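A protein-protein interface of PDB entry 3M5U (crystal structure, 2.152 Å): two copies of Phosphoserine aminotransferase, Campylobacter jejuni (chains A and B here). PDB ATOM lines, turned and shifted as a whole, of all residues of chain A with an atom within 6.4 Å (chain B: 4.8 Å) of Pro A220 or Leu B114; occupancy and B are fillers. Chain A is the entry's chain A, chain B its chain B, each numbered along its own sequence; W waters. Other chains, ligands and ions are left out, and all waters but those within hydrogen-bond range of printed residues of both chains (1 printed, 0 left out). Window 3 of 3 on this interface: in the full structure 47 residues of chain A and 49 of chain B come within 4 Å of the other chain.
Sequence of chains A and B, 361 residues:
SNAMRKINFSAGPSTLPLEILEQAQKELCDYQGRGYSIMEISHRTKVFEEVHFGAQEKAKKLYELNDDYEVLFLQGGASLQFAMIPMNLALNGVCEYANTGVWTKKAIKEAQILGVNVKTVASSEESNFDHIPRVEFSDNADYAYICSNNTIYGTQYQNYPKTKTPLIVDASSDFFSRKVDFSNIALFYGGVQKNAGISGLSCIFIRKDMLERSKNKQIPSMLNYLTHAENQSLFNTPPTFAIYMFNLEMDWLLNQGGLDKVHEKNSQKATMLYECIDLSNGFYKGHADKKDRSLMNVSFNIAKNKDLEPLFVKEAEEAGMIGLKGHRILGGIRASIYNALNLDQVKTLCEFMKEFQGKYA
Water W1 lies within hydrogen-bond range of N of Met A222, OE1 of Glu B110 and N of Ser A221.
Printed residues of chain B that touch a printed residue of chain A: Ala B83, Glu B110, Ile B113 and Leu B114.
Hydrophobic or aromatic side chains of chain B within 4 Å of the printed part of chain A: Ala B83, Ile B113 and Leu B114.
Along chain B the printed residues that touch a printed residue of chain A span positions 83 to 114.
Of the 9 printed residues of chain A, 4 touch a printed residue of chain B.
Among the printed residues, 7 pairs touch across the chains.
Among the printed residues, no Asp or Glu carboxylate lies within 4 Å of a Lys or Arg side-chain nitrogen of the other chain.
1 position is printed for both chains.
Of the 7 pairs that touch across the chains among the printed residues, none has its exchanged pair printed and touching as well.
Among the printed residues, merely in contact across the chains: Ile A219 with Ile B113 (3.5 Å), Pro A220 with Ala B83 (3.9 Å), Pro A220 with Glu B110 (3.1 Å), Pro A220 with Ile B113 (3.8 Å) and Pro A220 with Leu B114 (3.7 Å).
Of the printed residues of chain B, Gln A218 touches Ile B113 (3.3 Å).
Of chain B, only Ala B83 (3.9 Å), Glu B110 (3.1 Å), Ile B113 (3.8 Å) and Leu B114 (3.7 Å) come within 4 Å of Pro A220.
Met A222 touches none of the printed residues of chain B.
Of the printed residues of chain A, Ala B83 touches Pro A220.
Gln B112 touches none of the printed residues of chain A.
Of chain A, only Pro A220 comes within 4 Å of Leu B114.
The nearest printed residue of chain B that does not touch Pro A220 is Met B87 (5.0 Å).
The nearest printed residue of chain A that does not touch Glu B110 is Met A222 (4.7 Å).
The side-chain amide nitrogen of Gln A218 lies within hydrogen-bond range of the backbone carbonyl oxygen of Ile B113 (3.3 Å).
OE2 of Glu B110 is in hydrogen-bond range of OG of Ser A221 (2.6 Å).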
ATOM      1  N   MET A  87     -16.435 -14.479   5.893  1.00  0.00           N
ATOM      2  CA  MET A  87     -15.034 -14.155   5.653  1.00  0.00           C
ATOM      3  C   MET A  87     -14.687 -12.771   6.192  1.00  0.00           C
ATOM      4  O   MET A  87     -13.556 -12.522   6.607  1.00  0.00           O
ATOM      5  CB  MET A  87     -14.714 -14.234   4.159  1.00  0.00           C
ATOM      6  CG  MET A  87     -14.448 -15.642   3.654  1.00  0.00           C
ATOM      7  SD  MET A  87     -14.105 -15.702   1.736  1.00  0.00           S
ATOM      8  CE  MET A  87     -12.552 -14.525   1.668  1.00  0.00           C
ATOM      9  N   GLN A 218      -7.188 -10.501   6.747  1.00  0.00           N
ATOM     10  CA  GLN A 218      -6.250 -10.662   5.641  1.00  0.00           C
ATOM     11  C   GLN A 218      -6.763 -11.687   4.634  1.00  0.00           C
ATOM     12  O   GLN A 218      -6.372 -12.852   4.669  1.00  0.00           O
ATOM     13  CB  GLN A 218      -4.862 -11.047   6.145  1.00  0.00           C
ATOM     14  CG  GLN A 218      -3.791 -11.007   5.069  1.00  0.00           C
ATOM     15  CD  GLN A 218      -2.491 -11.641   5.531  1.00  0.00           C
ATOM     16  OE1 GLN A 218      -2.105 -11.507   6.698  1.00  0.00           O
ATOM     17  NE2 GLN A 218      -1.808 -12.341   4.619  1.00  0.00           N
ATOM     18  N   ILE A 219      -7.644 -11.232   3.747  1.00  0.00           N
ATOM     19  CA  ILE A 219      -8.279 -12.073   2.728  1.00  0.00           C
ATOM     20  C   ILE A 219      -8.067 -11.449   1.349  1.00  0.00           C
ATOM     21  O   ILE A 219      -7.786 -10.253   1.260  1.00  0.00           O
ATOM     22  CB  ILE A 219      -9.791 -12.169   2.983  1.00  0.00           C
ATOM     23  CG1 ILE A 219     -10.366 -10.758   3.184  1.00  0.00           C
ATOM     24  CG2 ILE A 219     -10.058 -13.062   4.186  1.00  0.00           C
ATOM     25  CD1 ILE A 219     -11.861 -10.713   3.529  1.00  0.00           C
ATOM     26  N   PRO A 220      -8.216 -12.245   0.277  1.00  0.00           N
ATOM     27  CA  PRO A 220      -8.082 -11.751  -1.092  1.00  0.00           C
ATOM     28  C   PRO A 220      -8.875 -10.470  -1.301  1.00  0.00           C
ATOM     29  O   PRO A 220     -10.010 -10.399  -0.861  1.00  0.00           O
ATOM     30  CB  PRO A 220      -8.717 -12.874  -1.919  1.00  0.00           C
ATOM     31  CG  PRO A 220      -8.442 -14.092  -1.125  1.00  0.00           C
ATOM     32  CD  PRO A 220      -8.654 -13.653   0.290  1.00  0.00           C
ATOM     33  N   SER A 221      -8.277  -9.489  -1.965  1.00  0.00           N
ATOM     34  CA  SER A 221      -8.961  -8.251  -2.326  1.00  0.00           C
ATOM     35  C   SER A 221     -10.373  -8.409  -2.856  1.00  0.00           C
ATOM     36  O   SER A 221     -11.295  -7.748  -2.393  1.00  0.00           O
ATOM     37  CB  SER A 221      -8.138  -7.527  -3.388  1.00  0.00           C
ATOM     38  OG  SER A 221      -6.814  -7.426  -2.936  1.00  0.00           O
ATOM     39  N   MET A 222     -10.545  -9.251  -3.860  1.00  0.00           N
ATOM     40  CA  MET A 222     -11.853  -9.376  -4.493  1.00  0.00           C
ATOM     41  C   MET A 222     -12.913  -9.816  -3.492  1.00  0.00           C
ATOM     42  O   MET A 222     -14.096  -9.569  -3.677  1.00  0.00           O
ATOM     43  CB  MET A 222     -11.767 -10.351  -5.666  1.00  0.00           C
ATOM     44  CG  MET A 222     -11.134  -9.686  -6.853  1.00  0.00           C
ATOM     45  SD  MET A 222     -12.310  -8.208  -7.410  1.00  0.00           S
ATOM     46  CE  MET A 222     -13.930  -9.365  -7.851  1.00  0.00           C
ATOM     47  N   LEU A 223     -12.472 -10.431  -2.402  1.00  0.00           N
ATOM     48  CA  LEU A 223     -13.407 -10.977  -1.417  1.00  0.00           C
ATOM     49  C   LEU A 223     -13.583 -10.062  -0.212  1.00  0.00           C
ATOM     50  O   LEU A 223     -14.368 -10.366   0.682  1.00  0.00           O
ATOM     51  CB  LEU A 223     -12.956 -12.387  -0.992  1.00  0.00           C
ATOM     52  CG  LEU A 223     -12.936 -13.381  -2.180  1.00  0.00           C
ATOM     53  CD1 LEU A 223     -12.450 -14.752  -1.753  1.00  0.00           C
ATOM     54  CD2 LEU A 223     -14.296 -13.486  -2.894  1.00  0.00           C
ATOM     55  N   ASN A 224     -12.845  -8.947  -0.217  1.00  0.00           N
ATOM     56  CA  ASN A 224     -12.790  -7.992   0.898  1.00  0.00           C
ATOM     57  C   ASN A 224     -13.731  -6.776   0.719  1.00  0.00           C
ATOM     58  O   ASN A 224     -13.533  -5.954  -0.180  1.00  0.00           O
ATOM     59  CB  ASN A 224     -11.337  -7.516   1.107  1.00  0.00           C
ATOM     60  CG  ASN A 224     -11.137  -6.842   2.467  1.00  0.00           C
ATOM     61  OD1 ASN A 224     -11.875  -5.938   2.832  1.00  0.00           O
ATOM     62  ND2 ASN A 224     -10.154  -7.313   3.230  1.00  0.00           N
ATOM     63  N   THR A 227     -12.025  -3.313   0.688  1.00  0.00           N
ATOM     64  CA  THR A 227     -11.369  -3.092  -0.605  1.00  0.00           C
ATOM     65  C   THR A 227     -12.337  -2.511  -1.646  1.00  0.00           C
ATOM     66  O   THR A 227     -12.016  -1.564  -2.354  1.00  0.00           O
ATOM     67  CB  THR A 227     -10.678  -4.385  -1.098  1.00  0.00           C
ATOM     68  OG1 THR A 227      -9.559  -4.664  -0.248  1.00  0.00           O
ATOM     69  CG2 THR A 227     -10.176  -4.245  -2.517  1.00  0.00           C
ATOM     70  N   ALA B  83      -7.433 -15.276  -7.120  1.00  0.00           N
ATOM     71  CA  ALA B  83      -7.672 -15.882  -5.836  1.00  0.00           C
ATOM     72  C   ALA B  83      -8.051 -17.352  -6.011  1.00  0.00           C
ATOM     73  O   ALA B  83      -7.518 -18.202  -5.302  1.00  0.00           O
ATOM     74  CB  ALA B  83      -8.789 -15.138  -5.114  1.00  0.00           C
ATOM     75  N   PRO B  86      -4.975 -20.078  -6.820  1.00  0.00           N
ATOM     76  CA  PRO B  86      -4.224 -20.787  -5.774  1.00  0.00           C
ATOM     77  C   PRO B  86      -5.128 -21.468  -4.712  1.00  0.00           C
ATOM     78  O   PRO B  86      -4.688 -22.410  -4.039  1.00  0.00           O
ATOM     79  CB  PRO B  86      -3.363 -19.680  -5.161  1.00  0.00           C
ATOM     80  CG  PRO B  86      -4.158 -18.417  -5.428  1.00  0.00           C
ATOM     81  CD  PRO B  86      -4.707 -18.630  -6.808  1.00  0.00           C
ATOM     82  N   MET B  87      -6.373 -21.023  -4.576  1.00  0.00           N
ATOM     83  CA  MET B  87      -7.271 -21.635  -3.584  1.00  0.00           C
ATOM     84  C   MET B  87      -7.586 -23.062  -3.973  1.00  0.00           C
ATOM     85  O   MET B  87      -7.703 -23.938  -3.117  1.00  0.00           O
ATOM     86  CB  MET B  87      -8.586 -20.857  -3.416  1.00  0.00           C
ATOM     87  CG  MET B  87      -8.451 -19.535  -2.636  1.00  0.00           C
ATOM     88  SD  MET B  87     -10.190 -18.637  -2.349  1.00  0.00           S
ATOM     89  CE  MET B  87     -11.119 -20.188  -1.651  1.00  0.00           C
ATOM     90  N   GLU B 110      -2.040 -11.621  -4.516  1.00  0.00           N
ATOM     91  CA  GLU B 110      -3.208 -12.337  -3.996  1.00  0.00           C
ATOM     92  C   GLU B 110      -2.846 -13.729  -3.501  1.00  0.00           C
ATOM     93  O   GLU B 110      -3.388 -14.191  -2.493  1.00  0.00           O
ATOM     94  CB  GLU B 110      -4.380 -12.383  -4.998  1.00  0.00           C
ATOM     95  CG  GLU B 110      -4.901 -11.018  -5.380  1.00  0.00           C
ATOM     96  CD  GLU B 110      -5.430 -10.204  -4.192  1.00  0.00           C
ATOM     97  OE1 GLU B 110      -6.164 -10.745  -3.345  1.00  0.00           O
ATOM     98  OE2 GLU B 110      -5.093  -9.014  -4.098  1.00  0.00           O
ATOM     99  N   ALA B 111      -1.928 -14.397  -4.193  1.00  0.00           N
ATOM    100  CA  ALA B 111      -1.493 -15.720  -3.752  1.00  0.00           C
ATOM    101  C   ALA B 111      -0.752 -15.638  -2.420  1.00  0.00           C
ATOM    102  O   ALA B 111      -0.947 -16.477  -1.544  1.00  0.00           O
ATOM    103  CB  ALA B 111      -0.624 -16.431  -4.838  1.00  0.00           C
ATOM    104  N   GLN B 112       0.103 -14.630  -2.283  1.00  0.00           N
ATOM    105  CA  GLN B 112       0.793 -14.357  -1.026  1.00  0.00           C
ATOM    106  C   GLN B 112      -0.191 -14.079   0.121  1.00  0.00           C
ATOM    107  O   GLN B 112      -0.021 -14.616   1.231  1.00  0.00           O
ATOM    108  CB  GLN B 112       1.777 -13.186  -1.198  1.00  0.00           C
ATOM    109  CG  GLN B 112       2.984 -13.547  -2.113  1.00  0.00           C
ATOM    110  CD  GLN B 112       3.838 -12.339  -2.521  1.00  0.00           C
ATOM    111  OE1 GLN B 112       3.340 -11.226  -2.653  1.00  0.00           O
ATOM    112  NE2 GLN B 112       5.132 -12.575  -2.746  1.00  0.00           N
ATOM    113  N   ILE B 113      -1.221 -13.265  -0.147  1.00  0.00           N
ATOM    114  CA  ILE B 113      -2.280 -13.027   0.845  1.00  0.00           C
ATOM    115  C   ILE B 113      -2.875 -14.344   1.360  1.00  0.00           C
ATOM    116  O   ILE B 113      -3.189 -14.459   2.551  1.00  0.00           O
ATOM    117  CB  ILE B 113      -3.408 -12.116   0.303  1.00  0.00           C
ATOM    118  CG1 ILE B 113      -2.881 -10.689   0.086  1.00  0.00           C
ATOM    119  CG2 ILE B 113      -4.596 -12.097   1.270  1.00  0.00           C
ATOM    120  CD1 ILE B 113      -3.747  -9.791  -0.841  1.00  0.00           C
ATOM    121  N   LEU B 114      -3.034 -15.330   0.469  1.00  0.00           N
ATOM    122  CA  LEU B 114      -3.583 -16.627   0.856  1.00  0.00           C
ATOM    123  C   LEU B 114      -2.489 -17.544   1.433  1.00  0.00           C
ATOM    124  O   LEU B 114      -2.712 -18.737   1.638  1.00  0.00           O
ATOM    125  CB  LEU B 114      -4.260 -17.320  -0.346  1.00  0.00           C
ATOM    126  CG  LEU B 114      -5.563 -16.716  -0.882  1.00  0.00           C
ATOM    127  CD1 LEU B 114      -5.722 -16.952  -2.378  1.00  0.00           C
ATOM    128  CD2 LEU B 114      -6.803 -17.194  -0.087  1.00  0.00           C
ATOM    129  N   GLY B 115      -1.302 -16.997   1.662  1.00  0.00           N
ATOM    130  CA  GLY B 115      -0.237 -17.753   2.298  1.00  0.00           C
ATOM    131  C   GLY B 115       0.273 -18.907   1.453  1.00  0.00           C
ATOM    132  O   GLY B 115       0.769 -19.901   1.981  1.00  0.00           O
ATOM    133  N   VAL B 116       0.131 -18.772   0.138  1.00  0.00           N
ATOM    134  CA  VAL B 116       0.694 -19.720  -0.823  1.00  0.00           C
ATOM    135  C   VAL B 116       2.214 -19.508  -0.907  1.00  0.00           C
ATOM    136  O   VAL B 116       2.682 -18.380  -0.805  1.00  0.00           O
ATOM    137  CB  VAL B 116       0.047 -19.519  -2.222  1.00  0.00           C
ATOM    138  CG1 VAL B 116       0.943 -20.078  -3.308  1.00  0.00           C
ATOM    139  CG2 VAL B 116      -1.374 -20.150  -2.259  1.00  0.00           C
HETATM  140  O   HOH W   1      -9.026 -11.269  -4.874  1.00  0.00           O
